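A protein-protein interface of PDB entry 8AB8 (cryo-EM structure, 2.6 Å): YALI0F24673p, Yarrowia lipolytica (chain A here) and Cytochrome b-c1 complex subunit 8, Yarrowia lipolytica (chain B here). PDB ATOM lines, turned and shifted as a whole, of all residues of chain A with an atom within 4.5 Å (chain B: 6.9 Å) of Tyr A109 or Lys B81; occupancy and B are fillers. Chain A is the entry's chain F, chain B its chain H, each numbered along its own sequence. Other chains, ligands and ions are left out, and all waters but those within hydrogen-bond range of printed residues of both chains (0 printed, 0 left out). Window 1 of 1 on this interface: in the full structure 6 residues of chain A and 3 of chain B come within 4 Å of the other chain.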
ATOM      1  N   CYS A  91      20.407 -11.784  40.523  1.00  0.00           N
ATOM      2  CA  CYS A  91      19.219 -11.313  39.819  1.00  0.00           C
ATOM      3  C   CYS A  91      17.990 -11.437  40.719  1.00  0.00           C
ATOM      4  O   CYS A  91      17.248 -10.472  40.875  1.00  0.00           O
ATOM      5  CB  CYS A  91      18.989 -12.020  38.482  1.00  0.00           C
ATOM      6  SG  CYS A  91      17.527 -11.423  37.578  1.00  0.00           S
ATOM      7  N   ARG A  94      17.795  -8.844  43.429  1.00  0.00           N
ATOM      8  CA  ARG A  94      17.446  -7.528  42.905  1.00  0.00           C
ATOM      9  C   ARG A  94      15.946  -7.432  42.630  1.00  0.00           C
ATOM     10  O   ARG A  94      15.329  -6.423  42.972  1.00  0.00           O
ATOM     11  CB  ARG A  94      18.237  -7.173  41.641  1.00  0.00           C
ATOM     12  CG  ARG A  94      19.740  -7.087  41.857  1.00  0.00           C
ATOM     13  CD  ARG A  94      20.574  -6.838  40.616  1.00  0.00           C
ATOM     14  NE  ARG A  94      20.546  -7.886  39.603  1.00  0.00           N
ATOM     15  CZ  ARG A  94      20.057  -7.739  38.376  1.00  0.00           C
ATOM     16  NH1 ARG A  94      19.516  -6.590  38.010  1.00  0.00           N
ATOM     17  NH2 ARG A  94      20.086  -8.744  37.516  1.00  0.00           N
ATOM     18  N   ALA A 107       5.013   0.593  37.373  1.00  0.00           N
ATOM     19  CA  ALA A 107       6.284   0.825  36.707  1.00  0.00           C
ATOM     20  C   ALA A 107       6.176   0.407  35.242  1.00  0.00           C
ATOM     21  O   ALA A 107       5.305  -0.379  34.875  1.00  0.00           O
ATOM     22  CB  ALA A 107       7.407   0.121  37.434  1.00  0.00           C
ATOM     23  N   GLU A 108       7.046   0.983  34.410  1.00  0.00           N
ATOM     24  CA  GLU A 108       7.034   0.716  32.984  1.00  0.00           C
ATOM     25  C   GLU A 108       7.695  -0.639  32.741  1.00  0.00           C
ATOM     26  O   GLU A 108       7.101  -1.521  32.119  1.00  0.00           O
ATOM     27  CB  GLU A 108       7.697   1.879  32.239  1.00  0.00           C
ATOM     28  CG  GLU A 108       7.448   1.883  30.736  1.00  0.00           C
ATOM     29  CD  GLU A 108       8.324   0.952  29.911  1.00  0.00           C
ATOM     30  OE1 GLU A 108       7.765   0.102  29.186  1.00  0.00           O
ATOM     31  OE2 GLU A 108       9.564   1.083  29.984  1.00  0.00           O
ATOM     32  N   TYR A 109       8.912  -0.786  33.277  1.00  0.00           N
ATOM     33  CA  TYR A 109       9.739  -1.962  33.073  1.00  0.00           C
ATOM     34  C   TYR A 109       9.827  -2.779  34.359  1.00  0.00           C
ATOM     35  O   TYR A 109      10.374  -2.308  35.359  1.00  0.00           O
ATOM     36  CB  TYR A 109      11.145  -1.560  32.614  1.00  0.00           C
ATOM     37  CG  TYR A 109      12.130  -2.699  32.530  1.00  0.00           C
ATOM     38  CD1 TYR A 109      11.939  -3.741  31.633  1.00  0.00           C
ATOM     39  CD2 TYR A 109      13.254  -2.741  33.346  1.00  0.00           C
ATOM     40  CE1 TYR A 109      12.837  -4.793  31.544  1.00  0.00           C
ATOM     41  CE2 TYR A 109      14.156  -3.794  33.280  1.00  0.00           C
ATOM     42  CZ  TYR A 109      13.947  -4.821  32.373  1.00  0.00           C
ATOM     43  OH  TYR A 109      14.838  -5.852  32.290  1.00  0.00           O
ATOM     44  N   LYS A 110       9.310  -4.009  34.297  1.00  0.00           N
ATOM     45  CA  LYS A 110       9.472  -4.964  35.382  1.00  0.00           C
ATOM     46  C   LYS A 110      10.491  -6.021  34.960  1.00  0.00           C
ATOM     47  O   LYS A 110      10.229  -6.818  34.057  1.00  0.00           O
ATOM     48  CB  LYS A 110       8.122  -5.565  35.792  1.00  0.00           C
ATOM     49  CG  LYS A 110       7.057  -4.564  36.207  1.00  0.00           C
ATOM     50  CD  LYS A 110       5.713  -5.202  36.455  1.00  0.00           C
ATOM     51  CE  LYS A 110       4.693  -4.253  37.053  1.00  0.00           C
ATOM     52  NZ  LYS A 110       4.826  -2.871  36.526  1.00  0.00           N
ATOM     53  N   GLU A 111      11.654  -6.013  35.624  1.00  0.00           N
ATOM     54  CA  GLU A 111      12.716  -6.977  35.383  1.00  0.00           C
ATOM     55  C   GLU A 111      12.299  -8.362  35.880  1.00  0.00           C
ATOM     56  O   GLU A 111      11.702  -8.482  36.947  1.00  0.00           O
ATOM     57  CB  GLU A 111      13.965  -6.539  36.151  1.00  0.00           C
ATOM     58  CG  GLU A 111      15.248  -7.101  35.560  1.00  0.00           C
ATOM     59  CD  GLU A 111      16.397  -7.301  36.535  1.00  0.00           C
ATOM     60  OE1 GLU A 111      17.113  -8.334  36.424  1.00  0.00           O
ATOM     61  OE2 GLU A 111      16.568  -6.432  37.414  1.00  0.00           O
ATOM     62  N   ASP A 112      12.642  -9.402  35.113  1.00  0.00           N
ATOM     63  CA  ASP A 112      12.555 -10.793  35.538  1.00  0.00           C
ATOM     64  C   ASP A 112      13.955 -11.397  35.551  1.00  0.00           C
ATOM     65  O   ASP A 112      14.938 -10.699  35.305  1.00  0.00           O
ATOM     66  CB  ASP A 112      11.628 -11.625  34.643  1.00  0.00           C
ATOM     67  CG  ASP A 112      11.924 -11.462  33.164  1.00  0.00           C
ATOM     68  OD1 ASP A 112      12.820 -12.164  32.658  1.00  0.00           O
ATOM     69  OD2 ASP A 112      11.279 -10.589  32.544  1.00  0.00           O
ATOM     70  N   GLU A 115      16.288 -14.705  31.824  1.00  0.00           N
ATOM     71  CA  GLU A 115      17.525 -14.776  31.060  1.00  0.00           C
ATOM     72  C   GLU A 115      18.606 -15.540  31.824  1.00  0.00           C
ATOM     73  O   GLU A 115      19.212 -16.464  31.272  1.00  0.00           O
ATOM     74  CB  GLU A 115      18.012 -13.382  30.692  1.00  0.00           C
ATOM     75  CG  GLU A 115      17.916 -13.094  29.213  1.00  0.00           C
ATOM     76  CD  GLU A 115      18.356 -11.686  28.838  1.00  0.00           C
ATOM     77  OE1 GLU A 115      19.560 -11.377  28.997  1.00  0.00           O
ATOM     78  OE2 GLU A 115      17.489 -10.892  28.401  1.00  0.00           O
ATOM     79  N   GLU A 116      18.819 -15.149  33.092  1.00  0.00           N
ATOM     80  CA  GLU A 116      19.869 -15.721  33.923  1.00  0.00           C
ATOM     81  C   GLU A 116      19.555 -17.182  34.229  1.00  0.00           C
ATOM     82  O   GLU A 116      20.458 -18.018  34.334  1.00  0.00           O
ATOM     83  CB  GLU A 116      20.000 -14.977  35.247  1.00  0.00           C
ATOM     84  CG  GLU A 116      20.766 -13.680  35.110  1.00  0.00           C
ATOM     85  CD  GLU A 116      19.904 -12.465  34.831  1.00  0.00           C
ATOM     86  OE1 GLU A 116      20.417 -11.326  35.000  1.00  0.00           O
ATOM     87  OE2 GLU A 116      18.707 -12.640  34.523  1.00  0.00           O
ATOM     88  N   TRP B  77      21.196 -10.002  20.402  1.00  0.00           N
ATOM     89  CA  TRP B  77      21.533  -9.054  21.446  1.00  0.00           C
ATOM     90  C   TRP B  77      20.385  -8.078  21.687  1.00  0.00           C
ATOM     91  O   TRP B  77      20.175  -7.631  22.813  1.00  0.00           O
ATOM     92  CB  TRP B  77      22.826  -8.320  21.089  1.00  0.00           C
ATOM     93  CG  TRP B  77      23.200  -7.336  22.149  1.00  0.00           C
ATOM     94  CD1 TRP B  77      23.822  -7.606  23.333  1.00  0.00           C
ATOM     95  CD2 TRP B  77      22.922  -5.928  22.148  1.00  0.00           C
ATOM     96  NE1 TRP B  77      23.975  -6.459  24.062  1.00  0.00           N
ATOM     97  CE2 TRP B  77      23.430  -5.414  23.363  1.00  0.00           C
ATOM     98  CE3 TRP B  77      22.304  -5.057  21.244  1.00  0.00           C
ATOM     99  CZ2 TRP B  77      23.342  -4.064  23.693  1.00  0.00           C
ATOM    100  CZ3 TRP B  77      22.222  -3.720  21.569  1.00  0.00           C
ATOM    101  CH2 TRP B  77      22.733  -3.236  22.777  1.00  0.00           C
ATOM    102  N   LEU B  78      19.653  -7.748  20.621  1.00  0.00           N
ATOM    103  CA  LEU B  78      18.581  -6.773  20.717  1.00  0.00           C
ATOM    104  C   LEU B  78      17.446  -7.314  21.583  1.00  0.00           C
ATOM    105  O   LEU B  78      16.678  -6.535  22.135  1.00  0.00           O
ATOM    106  CB  LEU B  78      18.071  -6.453  19.308  1.00  0.00           C
ATOM    107  CG  LEU B  78      18.876  -5.429  18.506  1.00  0.00           C
ATOM    108  CD1 LEU B  78      18.345  -5.332  17.081  1.00  0.00           C
ATOM    109  CD2 LEU B  78      18.864  -4.059  19.173  1.00  0.00           C
ATOM    110  N   TYR B  79      17.340  -8.647  21.681  1.00  0.00           N
ATOM    111  CA  TYR B  79      16.225  -9.273  22.376  1.00  0.00           C
ATOM    112  C   TYR B  79      16.661  -9.785  23.742  1.00  0.00           C
ATOM    113  O   TYR B  79      15.989 -10.623  24.341  1.00  0.00           O
ATOM    114  CB  TYR B  79      15.552 -10.332  21.497  1.00  0.00           C
ATOM    115  CG  TYR B  79      14.715  -9.708  20.416  1.00  0.00           C
ATOM    116  CD1 TYR B  79      13.382  -9.404  20.640  1.00  0.00           C
ATOM    117  CD2 TYR B  79      15.270  -9.358  19.193  1.00  0.00           C
ATOM    118  CE1 TYR B  79      12.610  -8.796  19.662  1.00  0.00           C
ATOM    119  CE2 TYR B  79      14.514  -8.746  18.203  1.00  0.00           C
ATOM    120  CZ  TYR B  79      13.180  -8.454  18.446  1.00  0.00           C
ATOM    121  OH  TYR B  79      12.420  -7.851  17.487  1.00  0.00           O
ATOM    122  N   THR B  80      17.793  -9.269  24.218  1.00  0.00           N
ATOM    123  CA  THR B  80      18.187  -9.466  25.601  1.00  0.00           C
ATOM    124  C   THR B  80      17.769  -8.236  26.396  1.00  0.00           C
ATOM    125  O   THR B  80      17.258  -7.279  25.816  1.00  0.00           O
ATOM    126  CB  THR B  80      19.679  -9.789  25.705  1.00  0.00           C
ATOM    127  OG1 THR B  80      20.413  -8.659  25.232  1.00  0.00           O
ATOM    128  CG2 THR B  80      20.051 -11.035  24.935  1.00  0.00           C
ATOM    129  N   LYS B  81      17.977  -8.296  27.718  1.00  0.00           N
ATOM    130  CA  LYS B  81      17.685  -7.211  28.640  1.00  0.00           C
ATOM    131  C   LYS B  81      18.583  -6.024  28.320  1.00  0.00           C
ATOM    132  O   LYS B  81      18.128  -4.884  28.311  1.00  0.00           O
ATOM    133  CB  LYS B  81      18.022  -7.631  30.074  1.00  0.00           C
ATOM    134  CG  LYS B  81      16.982  -8.458  30.809  1.00  0.00           C
ATOM    135  CD  LYS B  81      17.285  -8.514  32.299  1.00  0.00           C
ATOM    136  CE  LYS B  81      17.162  -9.900  32.897  1.00  0.00           C
ATOM    137  NZ  LYS B  81      17.749  -9.964  34.257  1.00  0.00           N
ATOM    138  N   ALA B  82      19.867  -6.325  28.070  1.00  0.00           N
ATOM    139  CA  ALA B  82      20.891  -5.345  27.750  1.00  0.00           C
ATOM    140  C   ALA B  82      20.532  -4.554  26.493  1.00  0.00           C
ATOM    141  O   ALA B  82      20.935  -3.397  26.359  1.00  0.00           O
ATOM    142  CB  ALA B  82      22.215  -6.046  27.593  1.00  0.00           C
ATOM    143  N   GLY B  83      19.774  -5.181  25.583  1.00  0.00           N
ATOM    144  CA  GLY B  83      19.507  -4.597  24.279  1.00  0.00           C
ATOM    145  C   GLY B  83      18.154  -3.900  24.191  1.00  0.00           C
ATOM    146  O   GLY B  83      17.693  -3.605  23.088  1.00  0.00           O
ATOM    147  N   ARG B  84      17.537  -3.674  25.359  1.00  0.00           N
ATOM    148  CA  ARG B  84      16.179  -3.168  25.484  1.00  0.00           C
ATOM    149  C   ARG B  84      16.024  -1.834  24.770  1.00  0.00           C
ATOM    150  O   ARG B  84      15.032  -1.601  24.079  1.00  0.00           O
ATOM    151  CB  ARG B  84      15.895  -2.825  26.943  1.00  0.00           C
ATOM    152  CG  ARG B  84      15.221  -3.945  27.713  1.00  0.00           C
ATOM    153  CD  ARG B  84      14.600  -3.337  28.939  1.00  0.00           C
ATOM    154  NE  ARG B  84      15.613  -2.892  29.883  1.00  0.00           N
ATOM    155  CZ  ARG B  84      15.484  -1.819  30.648  1.00  0.00           C
ATOM    156  NH1 ARG B  84      14.389  -1.082  30.579  1.00  0.00           N
ATOM    157  NH2 ARG B  84      16.451  -1.489  31.484  1.00  0.00           N
ATOM    158  N   HIS B  85      17.002  -0.957  25.010  1.00  0.00           N
ATOM    159  CA  HIS B  85      16.918   0.436  24.622  1.00  0.00           C
ATOM    160  C   HIS B  85      17.152   0.560  23.128  1.00  0.00           C
ATOM    161  O   HIS B  85      16.475   1.332  22.457  1.00  0.00           O
ATOM    162  CB  HIS B  85      17.950   1.260  25.391  1.00  0.00           C
ATOM    163  CG  HIS B  85      17.776   1.164  26.866  1.00  0.00           C
ATOM    164  ND1 HIS B  85      16.622   1.582  27.503  1.00  0.00           N
ATOM    165  CD2 HIS B  85      18.592   0.684  27.829  1.00  0.00           C
ATOM    166  CE1 HIS B  85      16.739   1.371  28.797  1.00  0.00           C
ATOM    167  NE2 HIS B  85      17.941   0.824  29.023  1.00  0.00           N
ATOM    168  N   GLU B  86      18.146  -0.193  22.647  1.00  0.00           N
ATOM    169  CA  GLU B  86      18.499  -0.228  21.241  1.00  0.00           C
ATOM    170  C   GLU B  86      17.371  -0.888  20.455  1.00  0.00           C
ATOM    171  O   GLU B  86      17.171  -0.549  19.291  1.00  0.00           O
ATOM    172  CB  GLU B  86      19.824  -0.960  21.021  1.00  0.00           C
ATOM    173  CG  GLU B  86      21.054  -0.167  21.430  1.00  0.00           C
ATOM    174  CD  GLU B  86      21.290   0.016  22.925  1.00  0.00           C
ATOM    175  OE1 GLU B  86      20.829  -0.838  23.722  1.00  0.00           O
ATOM    176  OE2 GLU B  86      21.922   1.026  23.293  1.00  0.00           O
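The guanidinium group of Arg A94 lies within salt-bridge range of the side-chain carboxylate of Glu A116 (3.6 Å). NH1 of Arg A94 is in salt-bridge range of OE2 of Glu A111 (3.0 Å). NH2 of Arg A94 lies close to SG of Cys A91, 3.7 Å away. The side-chain hydroxyl (OG1) of Thr B80 is in hydrogen-bond range of the backbone carbonyl oxygen (O) of Trp B77 (2.6 Å).
The side-chain carboxylate (OE2) of Glu A116 is in salt-bridge range of the side-chain amino group (NZ) of Lys B81 (2.9 Å). The side-chain amino group (NZ) of Lys B81 is in salt-bridge range of the side-chain carboxylate (OE1) of Glu A111, at 2.8 Å. The side-chain carboxylate (OE2) of Glu A115 is in hydrogen-bond range of the backbone NH (N) of Lys B81 (2.7 Å). NZ of Lys B81 sits at hydrogen-bond distance from SG of Cys A91 (3.6 Å). The side-chain amino group (NZ) of Lys B81 is in hydrogen-bond range of the backbone carbonyl oxygen (O) of Asp A112, at 3.1 Å.
Tyr A109 touches Lys B81 (OH to CD, 3.6 Å). CG of Tyr A109 touches NH1 of Arg B84, at 3.4 Å. OE2 of Glu A115 touches CA of Thr B80 (3.2 Å).
Of the 10 printed residues of chain A, 6 touch a printed residue of chain B. Hydrophobic or aromatic side chains of chain A within 4 Å of the printed part of chain B: Tyr A109.
Of the printed residues of chain B, Tyr A109 touches Lys B81 and Arg B84. Lys B81 touches just these residues of chain A: Cys A91, Tyr A109, Glu A111, Asp A112, Glu A115 and Glu A116. Of the printed residues of chain B, Glu A115 touches Thr B80 (3.2 Å) and Lys B81 (2.7 Å). Of the printed residues of chain B, Asp A112 touches Lys B81. Of the printed residues of chain B, Glu A116 touches Lys B81. Gly B83 touches none of the printed residues of chain A. The nearest residue of chain B that does not touch Tyr A109 is Ala B82 (6.6 Å).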
